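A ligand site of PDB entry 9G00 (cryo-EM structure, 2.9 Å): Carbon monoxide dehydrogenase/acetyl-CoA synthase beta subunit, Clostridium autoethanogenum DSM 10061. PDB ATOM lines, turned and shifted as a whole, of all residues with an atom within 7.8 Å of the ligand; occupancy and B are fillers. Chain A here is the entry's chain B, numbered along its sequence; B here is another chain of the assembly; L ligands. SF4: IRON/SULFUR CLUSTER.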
ATOM      1  N   GLN A  36     -23.813  11.952   6.452  1.00  0.00           N
ATOM      2  CA  GLN A  36     -24.498  10.685   6.608  1.00  0.00           C
ATOM      3  C   GLN A  36     -23.507   9.523   6.491  1.00  0.00           C
ATOM      4  O   GLN A  36     -22.446   9.621   5.866  1.00  0.00           O
ATOM      5  CB  GLN A  36     -25.641  10.577   5.599  1.00  0.00           C
ATOM      6  CG  GLN A  36     -26.772  11.571   5.914  1.00  0.00           C
ATOM      7  CD  GLN A  36     -27.894  11.535   4.876  1.00  0.00           C
ATOM      8  OE1 GLN A  36     -27.690  11.873   3.719  1.00  0.00           O
ATOM      9  NE2 GLN A  36     -29.093  11.115   5.298  1.00  0.00           N
ATOM     10  N   CYS A  37     -23.877   8.389   7.098  1.00  0.00           N
ATOM     11  CA  CYS A  37     -22.949   7.273   7.191  1.00  0.00           C
ATOM     12  C   CYS A  37     -22.491   6.809   5.809  1.00  0.00           C
ATOM     13  O   CYS A  37     -23.321   6.433   4.968  1.00  0.00           O
ATOM     14  CB  CYS A  37     -23.588   6.108   7.956  1.00  0.00           C
ATOM     15  SG  CYS A  37     -22.563   4.606   7.915  1.00  0.00           S
ATOM     16  N   GLY A  38     -21.182   6.723   5.625  1.00  0.00           N
ATOM     17  CA  GLY A  38     -20.638   6.310   4.342  1.00  0.00           C
ATOM     18  C   GLY A  38     -20.993   4.881   3.973  1.00  0.00           C
ATOM     19  O   GLY A  38     -21.301   4.591   2.818  1.00  0.00           O
ATOM     20  N   PHE A  39     -20.986   3.971   4.967  1.00  0.00           N
ATOM     21  CA  PHE A  39     -21.305   2.571   4.700  1.00  0.00           C
ATOM     22  C   PHE A  39     -22.739   2.432   4.198  1.00  0.00           C
ATOM     23  O   PHE A  39     -23.010   1.760   3.195  1.00  0.00           O
ATOM     24  CB  PHE A  39     -21.102   1.717   5.959  1.00  0.00           C
ATOM     25  CG  PHE A  39     -19.689   1.676   6.443  1.00  0.00           C
ATOM     26  CD1 PHE A  39     -18.737   0.915   5.774  1.00  0.00           C
ATOM     27  CD2 PHE A  39     -19.300   2.419   7.561  1.00  0.00           C
ATOM     28  CE1 PHE A  39     -17.400   0.870   6.209  1.00  0.00           C
ATOM     29  CE2 PHE A  39     -17.973   2.400   8.014  1.00  0.00           C
ATOM     30  CZ  PHE A  39     -17.016   1.617   7.335  1.00  0.00           C
ATOM     31  N   GLY A  40     -23.679   3.066   4.902  1.00  0.00           N
ATOM     32  CA  GLY A  40     -25.073   3.018   4.466  1.00  0.00           C
ATOM     33  C   GLY A  40     -25.287   3.717   3.136  1.00  0.00           C
ATOM     34  O   GLY A  40     -26.101   3.291   2.327  1.00  0.00           O
ATOM     35  N   SER A  41     -24.571   4.822   2.907  1.00  0.00           N
ATOM     36  CA  SER A  41     -24.705   5.544   1.647  1.00  0.00           C
ATOM     37  C   SER A  41     -24.219   4.691   0.472  1.00  0.00           C
ATOM     38  O   SER A  41     -24.811   4.729  -0.614  1.00  0.00           O
ATOM     39  CB  SER A  41     -23.934   6.867   1.692  1.00  0.00           C
ATOM     40  OG  SER A  41     -24.387   7.694   2.749  1.00  0.00           O
ATOM     41  N   ALA A  42     -23.161   3.903   0.668  1.00  0.00           N
ATOM     42  CA  ALA A  42     -22.678   3.028  -0.390  1.00  0.00           C
ATOM     43  C   ALA A  42     -23.409   1.689  -0.449  1.00  0.00           C
ATOM     44  O   ALA A  42     -23.220   0.936  -1.414  1.00  0.00           O
ATOM     45  CB  ALA A  42     -21.165   2.784  -0.234  1.00  0.00           C
ATOM     46  N   GLY A  43     -24.243   1.371   0.548  1.00  0.00           N
ATOM     47  CA  GLY A  43     -24.968   0.117   0.557  1.00  0.00           C
ATOM     48  C   GLY A  43     -24.174  -1.094   1.011  1.00  0.00           C
ATOM     49  O   GLY A  43     -24.611  -2.220   0.800  1.00  0.00           O
ATOM     50  N   VAL A  44     -23.017  -0.891   1.644  1.00  0.00           N
ATOM     51  CA  VAL A  44     -22.140  -1.967   2.095  1.00  0.00           C
ATOM     52  C   VAL A  44     -22.369  -2.330   3.557  1.00  0.00           C
ATOM     53  O   VAL A  44     -21.565  -3.063   4.148  1.00  0.00           O
ATOM     54  CB  VAL A  44     -20.665  -1.662   1.826  1.00  0.00           C
ATOM     55  CG1 VAL A  44     -20.346  -1.860   0.339  1.00  0.00           C
ATOM     56  CG2 VAL A  44     -20.289  -0.232   2.286  1.00  0.00           C
ATOM     57  N   CYS A  45     -23.427  -1.808   4.174  1.00  0.00           N
ATOM     58  CA  CYS A  45     -23.802  -2.201   5.530  1.00  0.00           C
ATOM     59  C   CYS A  45     -24.921  -3.223   5.458  1.00  0.00           C
ATOM     60  O   CYS A  45     -25.852  -3.071   4.654  1.00  0.00           O
ATOM     61  CB  CYS A  45     -24.266  -0.998   6.359  1.00  0.00           C
ATOM     62  SG  CYS A  45     -24.974  -1.472   7.968  1.00  0.00           S
ATOM     63  N   CYS A  46     -24.856  -4.242   6.308  1.00  0.00           N
ATOM     64  CA  CYS A  46     -25.871  -5.270   6.344  1.00  0.00           C
ATOM     65  C   CYS A  46     -26.360  -5.468   7.769  1.00  0.00           C
ATOM     66  O   CYS A  46     -25.583  -5.437   8.718  1.00  0.00           O
ATOM     67  CB  CYS A  46     -25.342  -6.607   5.794  1.00  0.00           C
ATOM     68  SG  CYS A  46     -26.644  -7.859   5.686  1.00  0.00           S
ATOM     69  N   ARG A  47     -27.678  -5.646   7.912  1.00  0.00           N
ATOM     70  CA  ARG A  47     -28.269  -5.938   9.221  1.00  0.00           C
ATOM     71  C   ARG A  47     -29.293  -7.066   9.109  1.00  0.00           C
ATOM     72  O   ARG A  47     -30.200  -7.158   9.937  1.00  0.00           O
ATOM     73  CB  ARG A  47     -28.913  -4.691   9.835  1.00  0.00           C
ATOM     74  CG  ARG A  47     -27.913  -3.557  10.100  1.00  0.00           C
ATOM     75  CD  ARG A  47     -28.502  -2.477  11.035  1.00  0.00           C
ATOM     76  NE  ARG A  47     -29.751  -1.949  10.504  1.00  0.00           N
ATOM     77  CZ  ARG A  47     -29.841  -0.840   9.781  1.00  0.00           C
ATOM     78  NH1 ARG A  47     -28.799  -0.074   9.541  1.00  0.00           N
ATOM     79  NH2 ARG A  47     -31.035  -0.487   9.281  1.00  0.00           N
ATOM     80  N   PRO A  53     -24.622  -6.152  13.296  1.00  0.00           N
ATOM     81  CA  PRO A  53     -24.429  -5.499  11.965  1.00  0.00           C
ATOM     82  C   PRO A  53     -23.044  -5.699  11.361  1.00  0.00           C
ATOM     83  O   PRO A  53     -22.053  -5.711  12.065  1.00  0.00           O
ATOM     84  CB  PRO A  53     -24.657  -3.991  12.264  1.00  0.00           C
ATOM     85  CG  PRO A  53     -25.244  -3.909  13.669  1.00  0.00           C
ATOM     86  CD  PRO A  53     -24.740  -5.150  14.380  1.00  0.00           C
ATOM     87  N   CYS A  54     -22.982  -5.879  10.023  1.00  0.00           N
ATOM     88  CA  CYS A  54     -21.727  -6.040   9.294  1.00  0.00           C
ATOM     89  C   CYS A  54     -21.572  -4.887   8.310  1.00  0.00           C
ATOM     90  O   CYS A  54     -22.529  -4.521   7.608  1.00  0.00           O
ATOM     91  CB  CYS A  54     -21.661  -7.376   8.519  1.00  0.00           C
ATOM     92  SG  CYS A  54     -21.641  -8.879   9.532  1.00  0.00           S
ATOM     93  N   ARG A  55     -20.385  -4.328   8.274  1.00  0.00           N
ATOM     94  CA  ARG A  55     -20.019  -3.343   7.274  1.00  0.00           C
ATOM     95  C   ARG A  55     -18.717  -3.786   6.624  1.00  0.00           C
ATOM     96  O   ARG A  55     -17.763  -4.161   7.316  1.00  0.00           O
ATOM     97  CB  ARG A  55     -19.905  -1.930   7.858  1.00  0.00           C
ATOM     98  CG  ARG A  55     -19.180  -1.843   9.169  1.00  0.00           C
ATOM     99  CD  ARG A  55     -19.450  -0.488   9.814  1.00  0.00           C
ATOM    100  NE  ARG A  55     -18.742  -0.401  11.081  1.00  0.00           N
ATOM    101  CZ  ARG A  55     -18.915   0.539  12.012  1.00  0.00           C
ATOM    102  NH1 ARG A  55     -19.803   1.498  11.849  1.00  0.00           N
ATOM    103  NH2 ARG A  55     -18.180   0.497  13.120  1.00  0.00           N
ATOM    104  N   GLN B  36     -18.860  -3.767  16.509  1.00  0.00           N
ATOM    105  CA  GLN B  36     -19.917  -3.564  15.531  1.00  0.00           C
ATOM    106  C   GLN B  36     -20.632  -2.225  15.771  1.00  0.00           C
ATOM    107  O   GLN B  36     -20.643  -1.691  16.887  1.00  0.00           O
ATOM    108  CB  GLN B  36     -20.896  -4.736  15.546  1.00  0.00           C
ATOM    109  CG  GLN B  36     -20.269  -6.020  14.986  1.00  0.00           C
ATOM    110  CD  GLN B  36     -21.204  -7.233  15.096  1.00  0.00           C
ATOM    111  OE1 GLN B  36     -21.595  -7.610  16.192  1.00  0.00           O
ATOM    112  NE2 GLN B  36     -21.565  -7.824  13.961  1.00  0.00           N
ATOM    113  N   CYS B  37     -21.236  -1.695  14.718  1.00  0.00           N
ATOM    114  CA  CYS B  37     -21.799  -0.356  14.794  1.00  0.00           C
ATOM    115  C   CYS B  37     -22.846  -0.259  15.894  1.00  0.00           C
ATOM    116  O   CYS B  37     -23.842  -0.998  15.889  1.00  0.00           O
ATOM    117  CB  CYS B  37     -22.409   0.039  13.441  1.00  0.00           C
ATOM    118  SG  CYS B  37     -23.320   1.618  13.544  1.00  0.00           S
ATOM    119  N   GLY B  38     -22.685   0.732  16.768  1.00  0.00           N
ATOM    120  CA  GLY B  38     -23.604   0.908  17.867  1.00  0.00           C
ATOM    121  C   GLY B  38     -25.017   1.265  17.427  1.00  0.00           C
ATOM    122  O   GLY B  38     -25.987   0.776  17.990  1.00  0.00           O
ATOM    123  N   PHE B  39     -25.141   2.112  16.389  1.00  0.00           N
ATOM    124  CA  PHE B  39     -26.455   2.506  15.905  1.00  0.00           C
ATOM    125  C   PHE B  39     -27.229   1.305  15.378  1.00  0.00           C
ATOM    126  O   PHE B  39     -28.399   1.097  15.729  1.00  0.00           O
ATOM    127  CB  PHE B  39     -26.333   3.559  14.796  1.00  0.00           C
ATOM    128  CG  PHE B  39     -25.712   4.851  15.234  1.00  0.00           C
ATOM    129  CD1 PHE B  39     -26.444   5.763  15.993  1.00  0.00           C
ATOM    130  CD2 PHE B  39     -24.398   5.149  14.889  1.00  0.00           C
ATOM    131  CE1 PHE B  39     -25.867   6.970  16.421  1.00  0.00           C
ATOM    132  CE2 PHE B  39     -23.794   6.356  15.310  1.00  0.00           C
ATOM    133  CZ  PHE B  39     -24.546   7.272  16.079  1.00  0.00           C
ATOM    134  N   GLY B  40     -26.581   0.484  14.545  1.00  0.00           N
ATOM    135  CA  GLY B  40     -27.235  -0.701  14.037  1.00  0.00           C
ATOM    136  C   GLY B  40     -27.515  -1.727  15.124  1.00  0.00           C
ATOM    137  O   GLY B  40     -28.534  -2.421  15.084  1.00  0.00           O
ATOM    138  N   SER B  41     -26.620  -1.831  16.103  1.00  0.00           N
ATOM    139  CA  SER B  41     -26.841  -2.779  17.204  1.00  0.00           C
ATOM    140  C   SER B  41     -28.051  -2.376  18.034  1.00  0.00           C
ATOM    141  O   SER B  41     -28.801  -3.234  18.499  1.00  0.00           O
ATOM    142  CB  SER B  41     -25.597  -2.871  18.093  1.00  0.00           C
ATOM    143  OG  SER B  41     -24.455  -3.286  17.345  1.00  0.00           O
ATOM    144  N   ALA B  42     -28.268  -1.074  18.228  1.00  0.00           N
ATOM    145  CA  ALA B  42     -29.432  -0.606  18.981  1.00  0.00           C
ATOM    146  C   ALA B  42     -30.687  -0.472  18.113  1.00  0.00           C
ATOM    147  O   ALA B  42     -31.778  -0.286  18.673  1.00  0.00           O
ATOM    148  CB  ALA B  42     -29.135   0.743  19.662  1.00  0.00           C
ATOM    149  N   GLY B  43     -30.565  -0.598  16.792  1.00  0.00           N
ATOM    150  CA  GLY B  43     -31.715  -0.480  15.910  1.00  0.00           C
ATOM    151  C   GLY B  43     -32.174   0.927  15.616  1.00  0.00           C
ATOM    152  O   GLY B  43     -33.290   1.112  15.117  1.00  0.00           O
ATOM    153  N   VAL B  44     -31.343   1.938  15.889  1.00  0.00           N
ATOM    154  CA  VAL B  44     -31.686   3.348  15.695  1.00  0.00           C
ATOM    155  C   VAL B  44     -31.157   3.886  14.362  1.00  0.00           C
ATOM    156  O   VAL B  44     -31.167   5.104  14.138  1.00  0.00           O
ATOM    157  CB  VAL B  44     -31.223   4.219  16.867  1.00  0.00           C
ATOM    158  CG1 VAL B  44     -32.164   4.037  18.051  1.00  0.00           C
ATOM    159  CG2 VAL B  44     -29.757   3.913  17.260  1.00  0.00           C
ATOM    160  N   CYS B  45     -30.679   3.011  13.476  1.00  0.00           N
ATOM    161  CA  CYS B  45     -30.286   3.406  12.135  1.00  0.00           C
ATOM    162  C   CYS B  45     -31.405   3.061  11.170  1.00  0.00           C
ATOM    163  O   CYS B  45     -32.006   1.990  11.269  1.00  0.00           O
ATOM    164  CB  CYS B  45     -28.998   2.714  11.682  1.00  0.00           C
ATOM    165  SG  CYS B  45     -28.608   2.995   9.925  1.00  0.00           S
ATOM    166  N   CYS B  46     -31.682   3.959  10.231  1.00  0.00           N
ATOM    167  CA  CYS B  46     -32.709   3.731   9.240  1.00  0.00           C
ATOM    168  C   CYS B  46     -32.159   3.959   7.834  1.00  0.00           C
ATOM    169  O   CYS B  46     -31.378   4.888   7.616  1.00  0.00           O
ATOM    170  CB  CYS B  46     -33.923   4.659   9.467  1.00  0.00           C
ATOM    171  SG  CYS B  46     -35.290   4.272   8.359  1.00  0.00           S
ATOM    172  N   ARG B  47     -32.553   3.099   6.907  1.00  0.00           N
ATOM    173  CA  ARG B  47     -32.168   3.266   5.503  1.00  0.00           C
ATOM    174  C   ARG B  47     -33.367   3.037   4.585  1.00  0.00           C
ATOM    175  O   ARG B  47     -33.192   2.690   3.412  1.00  0.00           O
ATOM    176  CB  ARG B  47     -31.017   2.328   5.124  1.00  0.00           C
ATOM    177  CG  ARG B  47     -29.737   2.595   5.925  1.00  0.00           C
ATOM    178  CD  ARG B  47     -28.515   1.911   5.277  1.00  0.00           C
ATOM    179  NE  ARG B  47     -28.734   0.468   5.123  1.00  0.00           N
ATOM    180  CZ  ARG B  47     -28.349  -0.451   5.993  1.00  0.00           C
ATOM    181  NH1 ARG B  47     -27.634  -0.138   7.056  1.00  0.00           N
ATOM    182  NH2 ARG B  47     -28.680  -1.728   5.781  1.00  0.00           N
ATOM    183  N   PRO B  53     -29.012   7.643   4.588  1.00  0.00           N
ATOM    184  CA  PRO B  53     -29.232   6.973   5.891  1.00  0.00           C
ATOM    185  C   PRO B  53     -29.391   7.922   7.079  1.00  0.00           C
ATOM    186  O   PRO B  53     -28.732   8.941   7.139  1.00  0.00           O
ATOM    187  CB  PRO B  53     -27.957   6.105   6.078  1.00  0.00           C
ATOM    188  CG  PRO B  53     -27.220   6.122   4.737  1.00  0.00           C
ATOM    189  CD  PRO B  53     -27.649   7.409   4.075  1.00  0.00           C
ATOM    190  N   CYS B  54     -30.290   7.591   8.014  1.00  0.00           N
ATOM    191  CA  CYS B  54     -30.512   8.374   9.227  1.00  0.00           C
ATOM    192  C   CYS B  54     -30.160   7.539  10.440  1.00  0.00           C
ATOM    193  O   CYS B  54     -30.529   6.364  10.528  1.00  0.00           O
ATOM    194  CB  CYS B  54     -31.968   8.870   9.352  1.00  0.00           C
ATOM    195  SG  CYS B  54     -32.527  10.036   8.096  1.00  0.00           S
ATOM    196  N   ARG B  55     -29.427   8.136  11.361  1.00  0.00           N
ATOM    197  CA  ARG B  55     -29.158   7.539  12.656  1.00  0.00           C
ATOM    198  C   ARG B  55     -29.541   8.552  13.726  1.00  0.00           C
ATOM    199  O   ARG B  55     -29.177   9.724  13.650  1.00  0.00           O
ATOM    200  CB  ARG B  55     -27.710   7.089  12.790  1.00  0.00           C
ATOM    201  CG  ARG B  55     -26.689   8.067  12.287  1.00  0.00           C
ATOM    202  CD  ARG B  55     -25.342   7.379  12.136  1.00  0.00           C
ATOM    203  NE  ARG B  55     -24.353   8.320  11.645  1.00  0.00           N
ATOM    204  CZ  ARG B  55     -23.139   8.008  11.203  1.00  0.00           C
ATOM    205  NH1 ARG B  55     -22.715   6.764  11.165  1.00  0.00           N
ATOM    206  NH2 ARG B  55     -22.341   8.987  10.773  1.00  0.00           N
HETATM  207 FE1  SF4 L   1     -23.823   3.059   9.030  1.00  0.00          FE
HETATM  208 FE2  SF4 L   1     -26.359   2.557   9.916  1.00  0.00          FE
HETATM  209 FE3  SF4 L   1     -24.206   1.846  11.456  1.00  0.00          FE
HETATM  210 FE4  SF4 L   1     -24.735   0.484   9.145  1.00  0.00          FE
HETATM  211  S1  SF4 L   1     -26.037   0.573  11.021  1.00  0.00           S
HETATM  212  S2  SF4 L   1     -22.707   1.230   9.848  1.00  0.00           S
HETATM  213  S3  SF4 L   1     -25.534   2.178   7.819  1.00  0.00           S
HETATM  214  S4  SF4 L   1     -24.838   3.971  10.862  1.00  0.00           S
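Of the 30 residues printed, 10 come within 4 Å of the ligand. The nearest printed residue that does not touch the ligand is Phe 39 of chain B (4.2 Å).
The backbone NH of Gly 40 of chain B sits close to a sulfur (S1) of the ligand, 3.6 Å away. A sulfur (S2) of the ligand lies close to the guanidinium group (NH1) of Arg 55 of chain A, at 3.5 Å. The side-chain sulfur (SG) of Cys 45 of chain B is bound to an iron atom (FE2) of the ligand (2.3 Å). The backbone NH (N) of Gly 40 of chain A sits close to a sulfur (S3) of the ligand (3.6 Å). A sulfur (S4) of the ligand sits close to the guanidinium group (NH1) of Arg 55 of chain B (3.5 Å). A sulfur (S1) of the ligand lies close to the guanidinium group (NH1) of Arg 47 of chain A (3.2 Å). SG of Cys 45 of chain A binds FE4 of the ligand, at 2.3 Å. The side-chain sulfur (SG) of Cys 37 of chain A is bound to an iron atom (FE1) of the ligand (2.3 Å). An iron atom (FE3) of the ligand is bound by the side-chain sulfur (SG) of Cys 37 of chain B (2.3 Å). NH1 of Arg 47 of chain B sits close to S3 of the ligand (3.2 Å).
SG of Cys 37 of chain B lies close to N of Phe 39 of chain B. The side-chain sulfur of Cys 37 of chain B lies close to the backbone NH of Gly 40 of chain B. The side-chain sulfur (SG) of Cys 37 of chain A lies close to the backbone NH (N) of Gly 40 of chain A (3.6 Å). The backbone carbonyl oxygen (O) of Cys 37 of chain B sits at hydrogen-bond distance from the side-chain hydroxyl (OG) of Ser 41 of chain B, at 2.8 Å. SG of Cys 37 of chain A lies close to N of Phe 39 of chain A. The guanidinium group (NH1) of Arg 47 of chain B sits close to the guanidinium group (NH1) of Arg 47 of chain A (2.7 Å). O of Cys 37 of chain A sits at hydrogen-bond distance from OG of Ser 41 of chain A, at 2.8 Å. O of Cys 45 of chain B is in hydrogen-bond range of NH2 of Arg 47 of chain A (3.3 Å).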
